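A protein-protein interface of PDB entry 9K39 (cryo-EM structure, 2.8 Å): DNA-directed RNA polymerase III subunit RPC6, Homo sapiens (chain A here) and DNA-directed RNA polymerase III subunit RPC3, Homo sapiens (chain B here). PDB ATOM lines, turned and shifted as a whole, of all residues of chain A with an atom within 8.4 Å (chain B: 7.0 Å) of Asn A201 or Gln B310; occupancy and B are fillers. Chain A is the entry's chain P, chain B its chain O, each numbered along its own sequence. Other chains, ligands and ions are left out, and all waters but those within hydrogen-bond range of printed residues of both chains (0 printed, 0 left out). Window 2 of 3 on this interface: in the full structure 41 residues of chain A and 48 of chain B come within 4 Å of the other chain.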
ATOM      1  N   ALA A 195      29.791 -22.245  16.781  1.00  0.00           N
ATOM      2  CA  ALA A 195      28.334 -22.232  16.761  1.00  0.00           C
ATOM      3  C   ALA A 195      27.794 -22.740  15.430  1.00  0.00           C
ATOM      4  O   ALA A 195      26.800 -23.476  15.394  1.00  0.00           O
ATOM      5  CB  ALA A 195      27.819 -20.820  17.045  1.00  0.00           C
ATOM      6  N   ARG A 196      28.435 -22.357  14.324  1.00  0.00           N
ATOM      7  CA  ARG A 196      27.994 -22.822  13.014  1.00  0.00           C
ATOM      8  C   ARG A 196      28.230 -24.316  12.848  1.00  0.00           C
ATOM      9  O   ARG A 196      27.365 -25.036  12.335  1.00  0.00           O
ATOM     10  CB  ARG A 196      28.708 -22.038  11.912  1.00  0.00           C
ATOM     11  CG  ARG A 196      28.328 -22.459  10.501  1.00  0.00           C
ATOM     12  CD  ARG A 196      29.076 -21.654   9.443  1.00  0.00           C
ATOM     13  NE  ARG A 196      28.703 -20.242   9.450  1.00  0.00           N
ATOM     14  CZ  ARG A 196      29.432 -19.277  10.001  1.00  0.00           C
ATOM     15  NH1 ARG A 196      30.582 -19.567  10.594  1.00  0.00           N
ATOM     16  NH2 ARG A 196      29.012 -18.019   9.957  1.00  0.00           N
ATOM     17  N   SER A 198      28.323 -26.479  15.183  1.00  0.00           N
ATOM     18  CA  SER A 198      27.474 -27.237  16.096  1.00  0.00           C
ATOM     19  C   SER A 198      26.192 -27.693  15.407  1.00  0.00           C
ATOM     20  O   SER A 198      25.741 -28.826  15.613  1.00  0.00           O
ATOM     21  CB  SER A 198      27.151 -26.398  17.333  1.00  0.00           C
ATOM     22  OG  SER A 198      26.477 -25.203  16.978  1.00  0.00           O
ATOM     23  N   LYS A 199      25.591 -26.814  14.599  1.00  0.00           N
ATOM     24  CA  LYS A 199      24.393 -27.070  13.797  1.00  0.00           C
ATOM     25  C   LYS A 199      23.315 -27.841  14.557  1.00  0.00           C
ATOM     26  O   LYS A 199      22.591 -28.653  13.969  1.00  0.00           O
ATOM     27  CB  LYS A 199      24.757 -27.793  12.490  1.00  0.00           C
ATOM     28  CG  LYS A 199      25.313 -29.208  12.617  1.00  0.00           C
ATOM     29  CD  LYS A 199      25.629 -29.800  11.251  1.00  0.00           C
ATOM     30  CE  LYS A 199      26.164 -31.216  11.374  1.00  0.00           C
ATOM     31  NZ  LYS A 199      25.183 -32.126  12.028  1.00  0.00           N
ATOM     32  N   GLN A 200      23.186 -27.580  15.859  1.00  0.00           N
ATOM     33  CA  GLN A 200      22.172 -28.269  16.652  1.00  0.00           C
ATOM     34  C   GLN A 200      20.790 -27.670  16.416  1.00  0.00           C
ATOM     35  O   GLN A 200      19.820 -28.398  16.176  1.00  0.00           O
ATOM     36  CB  GLN A 200      22.548 -28.217  18.135  1.00  0.00           C
ATOM     37  CG  GLN A 200      21.689 -29.091  19.036  1.00  0.00           C
ATOM     38  CD  GLN A 200      20.484 -28.358  19.594  1.00  0.00           C
ATOM     39  OE1 GLN A 200      20.443 -27.131  19.606  1.00  0.00           O
ATOM     40  NE2 GLN A 200      19.496 -29.114  20.059  1.00  0.00           N
ATOM     41  N   ASN A 201      20.683 -26.343  16.478  1.00  0.00           N
ATOM     42  CA  ASN A 201      19.426 -25.638  16.250  1.00  0.00           C
ATOM     43  C   ASN A 201      19.719 -24.169  15.975  1.00  0.00           C
ATOM     44  O   ASN A 201      20.559 -23.568  16.657  1.00  0.00           O
ATOM     45  CB  ASN A 201      18.494 -25.788  17.454  1.00  0.00           C
ATOM     46  CG  ASN A 201      17.122 -25.188  17.209  1.00  0.00           C
ATOM     47  OD1 ASN A 201      16.228 -25.849  16.684  1.00  0.00           O
ATOM     48  ND2 ASN A 201      16.950 -23.927  17.595  1.00  0.00           N
ATOM     49  N   PRO A 202      19.051 -23.556  14.989  1.00  0.00           N
ATOM     50  CA  PRO A 202      19.384 -22.164  14.631  1.00  0.00           C
ATOM     51  C   PRO A 202      19.316 -21.193  15.797  1.00  0.00           C
ATOM     52  O   PRO A 202      20.184 -20.319  15.919  1.00  0.00           O
ATOM     53  CB  PRO A 202      18.348 -21.830  13.550  1.00  0.00           C
ATOM     54  CG  PRO A 202      17.992 -23.152  12.956  1.00  0.00           C
ATOM     55  CD  PRO A 202      18.032 -24.130  14.093  1.00  0.00           C
ATOM     56  N   MET A 203      18.307 -21.319  16.662  1.00  0.00           N
ATOM     57  CA  MET A 203      18.247 -20.473  17.850  1.00  0.00           C
ATOM     58  C   MET A 203      19.424 -20.751  18.777  1.00  0.00           C
ATOM     59  O   MET A 203      20.064 -19.824  19.286  1.00  0.00           O
ATOM     60  CB  MET A 203      16.920 -20.685  18.582  1.00  0.00           C
ATOM     61  CG  MET A 203      15.710 -20.176  17.820  1.00  0.00           C
ATOM     62  SD  MET A 203      15.822 -18.410  17.483  1.00  0.00           S
ATOM     63  CE  MET A 203      14.293 -18.140  16.595  1.00  0.00           C
ATOM     64  N   ILE A 204      19.724 -22.032  19.002  1.00  0.00           N
ATOM     65  CA  ILE A 204      20.861 -22.396  19.843  1.00  0.00           C
ATOM     66  C   ILE A 204      22.165 -21.940  19.200  1.00  0.00           C
ATOM     67  O   ILE A 204      23.080 -21.473  19.888  1.00  0.00           O
ATOM     68  CB  ILE A 204      20.857 -23.911  20.122  1.00  0.00           C
ATOM     69  CG1 ILE A 204      19.881 -24.259  21.254  1.00  0.00           C
ATOM     70  CG2 ILE A 204      22.256 -24.412  20.457  1.00  0.00           C
ATOM     71  CD1 ILE A 204      18.421 -24.282  20.847  1.00  0.00           C
ATOM     72  N   GLN A 205      22.266 -22.052  17.874  1.00  0.00           N
ATOM     73  CA  GLN A 205      23.458 -21.581  17.173  1.00  0.00           C
ATOM     74  C   GLN A 205      23.651 -20.081  17.366  1.00  0.00           C
ATOM     75  O   GLN A 205      24.762 -19.615  17.641  1.00  0.00           O
ATOM     76  CB  GLN A 205      23.370 -21.925  15.687  1.00  0.00           C
ATOM     77  CG  GLN A 205      23.400 -23.410  15.379  1.00  0.00           C
ATOM     78  CD  GLN A 205      23.078 -23.710  13.928  1.00  0.00           C
ATOM     79  OE1 GLN A 205      22.299 -24.612  13.629  1.00  0.00           O
ATOM     80  NE2 GLN A 205      23.680 -22.950  13.020  1.00  0.00           N
ATOM     81  N   ARG A 206      22.571 -19.306  17.220  1.00  0.00           N
ATOM     82  CA  ARG A 206      22.672 -17.861  17.393  1.00  0.00           C
ATOM     83  C   ARG A 206      23.008 -17.495  18.834  1.00  0.00           C
ATOM     84  O   ARG A 206      23.785 -16.565  19.077  1.00  0.00           O
ATOM     85  CB  ARG A 206      21.371 -17.187  16.955  1.00  0.00           C
ATOM     86  CG  ARG A 206      21.112 -17.250  15.458  1.00  0.00           C
ATOM     87  CD  ARG A 206      22.227 -16.571  14.678  1.00  0.00           C
ATOM     88  NE  ARG A 206      22.361 -15.161  15.027  1.00  0.00           N
ATOM     89  CZ  ARG A 206      21.732 -14.172  14.397  1.00  0.00           C
ATOM     90  NH1 ARG A 206      20.924 -14.440  13.382  1.00  0.00           N
ATOM     91  NH2 ARG A 206      21.914 -12.917  14.782  1.00  0.00           N
ATOM     92  N   ASN A 207      22.430 -18.209  19.805  1.00  0.00           N
ATOM     93  CA  ASN A 207      22.717 -17.915  21.204  1.00  0.00           C
ATOM     94  C   ASN A 207      24.160 -18.259  21.561  1.00  0.00           C
ATOM     95  O   ASN A 207      24.800 -17.542  22.339  1.00  0.00           O
ATOM     96  CB  ASN A 207      21.743 -18.664  22.113  1.00  0.00           C
ATOM     97  CG  ASN A 207      20.328 -18.134  22.010  1.00  0.00           C
ATOM     98  OD1 ASN A 207      19.373 -18.900  21.859  1.00  0.00           O
ATOM     99  ND2 ASN A 207      20.180 -16.817  22.091  1.00  0.00           N
ATOM    100  N   SER A 208      24.687 -19.353  21.007  1.00  0.00           N
ATOM    101  CA  SER A 208      26.068 -19.728  21.282  1.00  0.00           C
ATOM    102  C   SER A 208      27.053 -18.819  20.557  1.00  0.00           C
ATOM    103  O   SER A 208      28.152 -18.572  21.067  1.00  0.00           O
ATOM    104  CB  SER A 208      26.303 -21.188  20.893  1.00  0.00           C
ATOM    105  OG  SER A 208      25.884 -21.435  19.562  1.00  0.00           O
ATOM    106  N   LYS B 305       8.197 -27.460   9.824  1.00  0.00           N
ATOM    107  CA  LYS B 305       7.428 -26.232  10.010  1.00  0.00           C
ATOM    108  C   LYS B 305       8.022 -25.365  11.115  1.00  0.00           C
ATOM    109  O   LYS B 305       8.104 -24.136  10.973  1.00  0.00           O
ATOM    110  CB  LYS B 305       5.974 -26.578  10.323  1.00  0.00           C
ATOM    111  CG  LYS B 305       5.056 -25.377  10.475  1.00  0.00           C
ATOM    112  CD  LYS B 305       4.963 -24.586   9.182  1.00  0.00           C
ATOM    113  CE  LYS B 305       3.893 -23.513   9.275  1.00  0.00           C
ATOM    114  NZ  LYS B 305       4.112 -22.610  10.439  1.00  0.00           N
ATOM    115  N   GLN B 306       8.451 -25.982  12.218  1.00  0.00           N
ATOM    116  CA  GLN B 306       9.001 -25.209  13.325  1.00  0.00           C
ATOM    117  C   GLN B 306      10.337 -24.573  12.958  1.00  0.00           C
ATOM    118  O   GLN B 306      10.644 -23.473  13.431  1.00  0.00           O
ATOM    119  CB  GLN B 306       9.142 -26.093  14.567  1.00  0.00           C
ATOM    120  CG  GLN B 306       9.996 -27.338  14.376  1.00  0.00           C
ATOM    121  CD  GLN B 306      11.446 -27.122  14.767  1.00  0.00           C
ATOM    122  OE1 GLN B 306      11.830 -26.037  15.200  1.00  0.00           O
ATOM    123  NE2 GLN B 306      12.257 -28.163  14.622  1.00  0.00           N
ATOM    124  N   VAL B 307      11.132 -25.235  12.113  1.00  0.00           N
ATOM    125  CA  VAL B 307      12.391 -24.642  11.670  1.00  0.00           C
ATOM    126  C   VAL B 307      12.124 -23.401  10.826  1.00  0.00           C
ATOM    127  O   VAL B 307      12.806 -22.377  10.967  1.00  0.00           O
ATOM    128  CB  VAL B 307      13.232 -25.679  10.904  1.00  0.00           C
ATOM    129  CG1 VAL B 307      14.541 -25.060  10.435  1.00  0.00           C
ATOM    130  CG2 VAL B 307      13.497 -26.895  11.776  1.00  0.00           C
ATOM    131  N   LEU B 308      11.120 -23.466   9.946  1.00  0.00           N
ATOM    132  CA  LEU B 308      10.755 -22.293   9.158  1.00  0.00           C
ATOM    133  C   LEU B 308      10.221 -21.177  10.046  1.00  0.00           C
ATOM    134  O   LEU B 308      10.519 -19.998   9.822  1.00  0.00           O
ATOM    135  CB  LEU B 308       9.722 -22.673   8.097  1.00  0.00           C
ATOM    136  CG  LEU B 308       9.134 -21.511   7.292  1.00  0.00           C
ATOM    137  CD1 LEU B 308      10.222 -20.772   6.529  1.00  0.00           C
ATOM    138  CD2 LEU B 308       8.050 -22.002   6.344  1.00  0.00           C
ATOM    139  N   ASP B 309       9.426 -21.530  11.060  1.00  0.00           N
ATOM    140  CA  ASP B 309       8.922 -20.519  11.986  1.00  0.00           C
ATOM    141  C   ASP B 309      10.067 -19.837  12.724  1.00  0.00           C
ATOM    142  O   ASP B 309      10.074 -18.609  12.880  1.00  0.00           O
ATOM    143  CB  ASP B 309       7.941 -21.159  12.968  1.00  0.00           C
ATOM    144  CG  ASP B 309       7.047 -20.137  13.657  1.00  0.00           C
ATOM    145  OD1 ASP B 309       7.553 -19.079  14.084  1.00  0.00           O
ATOM    146  OD2 ASP B 309       5.830 -20.399  13.768  1.00  0.00           O
ATOM    147  N   GLN B 310      11.047 -20.619  13.185  1.00  0.00           N
ATOM    148  CA  GLN B 310      12.205 -20.046  13.863  1.00  0.00           C
ATOM    149  C   GLN B 310      13.001 -19.148  12.923  1.00  0.00           C
ATOM    150  O   GLN B 310      13.438 -18.057  13.311  1.00  0.00           O
ATOM    151  CB  GLN B 310      13.091 -21.160  14.426  1.00  0.00           C
ATOM    152  CG  GLN B 310      12.464 -21.929  15.577  1.00  0.00           C
ATOM    153  CD  GLN B 310      13.346 -23.057  16.075  1.00  0.00           C
ATOM    154  OE1 GLN B 310      14.442 -23.277  15.559  1.00  0.00           O
ATOM    155  NE2 GLN B 310      12.874 -23.775  17.085  1.00  0.00           N
ATOM    156  N   TYR B 311      13.203 -19.592  11.680  1.00  0.00           N
ATOM    157  CA  TYR B 311      13.916 -18.774  10.703  1.00  0.00           C
ATOM    158  C   TYR B 311      13.209 -17.443  10.481  1.00  0.00           C
ATOM    159  O   TYR B 311      13.843 -16.383  10.475  1.00  0.00           O
ATOM    160  CB  TYR B 311      14.056 -19.536   9.383  1.00  0.00           C
ATOM    161  CG  TYR B 311      15.207 -20.514   9.351  1.00  0.00           C
ATOM    162  CD1 TYR B 311      16.326 -20.327  10.152  1.00  0.00           C
ATOM    163  CD2 TYR B 311      15.179 -21.622   8.515  1.00  0.00           C
ATOM    164  CE1 TYR B 311      17.383 -21.216  10.123  1.00  0.00           C
ATOM    165  CE2 TYR B 311      16.229 -22.519   8.478  1.00  0.00           C
ATOM    166  CZ  TYR B 311      17.328 -22.309   9.284  1.00  0.00           C
ATOM    167  OH  TYR B 311      18.379 -23.200   9.251  1.00  0.00           O
ATOM    168  N   LEU B 312      11.886 -17.479  10.312  1.00  0.00           N
ATOM    169  CA  LEU B 312      11.138 -16.251  10.063  1.00  0.00           C
ATOM    170  C   LEU B 312      11.167 -15.324  11.269  1.00  0.00           C
ATOM    171  O   LEU B 312      11.343 -14.108  11.123  1.00  0.00           O
ATOM    172  CB  LEU B 312       9.698 -16.586   9.670  1.00  0.00           C
ATOM    173  CG  LEU B 312       9.522 -17.293   8.322  1.00  0.00           C
ATOM    174  CD1 LEU B 312       8.059 -17.639   8.080  1.00  0.00           C
ATOM    175  CD2 LEU B 312      10.065 -16.437   7.191  1.00  0.00           C
ATOM    176  N   THR B 313      11.007 -15.874  12.478  1.00  0.00           N
ATOM    177  CA  THR B 313      10.975 -15.025  13.664  1.00  0.00           C
ATOM    178  C   THR B 313      12.357 -14.507  14.042  1.00  0.00           C
ATOM    179  O   THR B 313      12.460 -13.498  14.746  1.00  0.00           O
ATOM    180  CB  THR B 313      10.347 -15.770  14.844  1.00  0.00           C
ATOM    181  OG1 THR B 313      10.078 -14.845  15.906  1.00  0.00           O
ATOM    182  CG2 THR B 313      11.272 -16.854  15.362  1.00  0.00           C
ATOM    183  N   LEU B 314      13.429 -15.171  13.593  1.00  0.00           N
ATOM    184  CA  LEU B 314      14.762 -14.623  13.816  1.00  0.00           C
ATOM    185  C   LEU B 314      15.140 -13.614  12.738  1.00  0.00           C
ATOM    186  O   LEU B 314      15.904 -12.681  13.010  1.00  0.00           O
ATOM    187  CB  LEU B 314      15.801 -15.750  13.899  1.00  0.00           C
ATOM    188  CG  LEU B 314      16.328 -16.470  12.656  1.00  0.00           C
ATOM    189  CD1 LEU B 314      17.565 -15.781  12.094  1.00  0.00           C
ATOM    190  CD2 LEU B 314      16.642 -17.922  12.983  1.00  0.00           C
ATOM    191  N   LEU B 315      14.628 -13.785  11.515  1.00  0.00           N
ATOM    192  CA  LEU B 315      14.817 -12.765  10.491  1.00  0.00           C
ATOM    193  C   LEU B 315      14.028 -11.503  10.807  1.00  0.00           C
ATOM    194  O   LEU B 315      14.468 -10.397  10.469  1.00  0.00           O
ATOM    195  CB  LEU B 315      14.418 -13.310   9.121  1.00  0.00           C
ATOM    196  CG  LEU B 315      15.535 -13.798   8.193  1.00  0.00           C
ATOM    197  CD1 LEU B 315      16.273 -14.985   8.789  1.00  0.00           C
ATOM    198  CD2 LEU B 315      14.972 -14.148   6.821  1.00  0.00           C
ATOM    199  N   ALA B 316      12.865 -11.646  11.451  1.00  0.00           N
ATOM    200  CA  ALA B 316      12.083 -10.473  11.828  1.00  0.00           C
ATOM    201  C   ALA B 316      12.773  -9.664  12.919  1.00  0.00           C
ATOM    202  O   ALA B 316      12.571  -8.447  13.010  1.00  0.00           O
ATOM    203  CB  ALA B 316      10.685 -10.896  12.281  1.00  0.00           C
ATOM    204  N   TYR B 334       4.187 -13.081   7.445  1.00  0.00           N
ATOM    205  CA  TYR B 334       5.387 -12.268   7.331  1.00  0.00           C
ATOM    206  C   TYR B 334       5.385 -11.515   6.009  1.00  0.00           C
ATOM    207  O   TYR B 334       4.749 -11.933   5.038  1.00  0.00           O
ATOM    208  CB  TYR B 334       6.660 -13.118   7.447  1.00  0.00           C
ATOM    209  CG  TYR B 334       6.940 -13.616   8.850  1.00  0.00           C
ATOM    210  CD1 TYR B 334       7.815 -12.935   9.688  1.00  0.00           C
ATOM    211  CD2 TYR B 334       6.327 -14.764   9.335  1.00  0.00           C
ATOM    212  CE1 TYR B 334       8.075 -13.386  10.968  1.00  0.00           C
ATOM    213  CE2 TYR B 334       6.579 -15.221  10.615  1.00  0.00           C
ATOM    214  CZ  TYR B 334       7.452 -14.528  11.427  1.00  0.00           C
ATOM    215  OH  TYR B 334       7.706 -14.981  12.700  1.00  0.00           O
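Among the printed residues, merely in contact across the chains: Pro A202 with Gln B310, Pro A202 with Tyr B311, Met A203 with Gln B310, Met A203 with Thr B313, Met A203 with Leu B314 and Arg A206 with Leu B314.
The side-chain amide oxygen (OE1) of Gln B310 lies within hydrogen-bond range of the side-chain amide nitrogen (ND2) of Asn A201 (3.3 Å).
Asn A201 touches just one residue of chain B: Gln B310.
Printed residues of chain B within 4 Å of Met A203: Gln B310, Thr B313 and Leu B314.
Gln B310 touches three residues of chain A.
Of the printed residues of chain A, Tyr B311 touches Pro A202.
Of the printed residues of chain A, Thr B313 touches Met A203 (3.5 Å).
Printed residues of chain A within 4 Å of Leu B314: Met A203 and Arg A206.
The nearest residue of chain B that does not touch Asn A201 is Gln B306 (4.6 Å).
The nearest residue of chain A that does not touch Gln B310 is Ile A204 (6.4 Å).
The nearest printed residue of chain A that does not touch Thr B313 is Arg A206 (8.6 Å).
Hydrophobic or aromatic side chains of chain B within 4 Å of the printed part of chain A: Tyr B311 and Leu B314.
Printed residues of chain A that touch a printed residue of chain B: Asn A201, Pro A202, Met A203 and Arg A206.
Hydrophobic or aromatic side chains of chain A that line the printed part of chain B: Pro A202 and Met A203.
Along chain A the printed residues that touch a printed residue of chain B span positions 201 to 206.
The backbone NH of Thr B313 lies close to the side-chain hydroxyl of Tyr B334.
The side-chain amide oxygen (OE1) of Gln B306 is in hydrogen-bond range of the side-chain amide nitrogen (NE2) of Gln B310, 3.1 Å away.
The side-chain amide nitrogen (ND2) of Asn A201 lies close to the backbone NH (N) of Met A203 (3.1 Å).
The backbone carbonyl oxygen (O) of Met A203 lies close to the side-chain amide oxygen (OD1) of Asn A207, 2.8 Å away.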
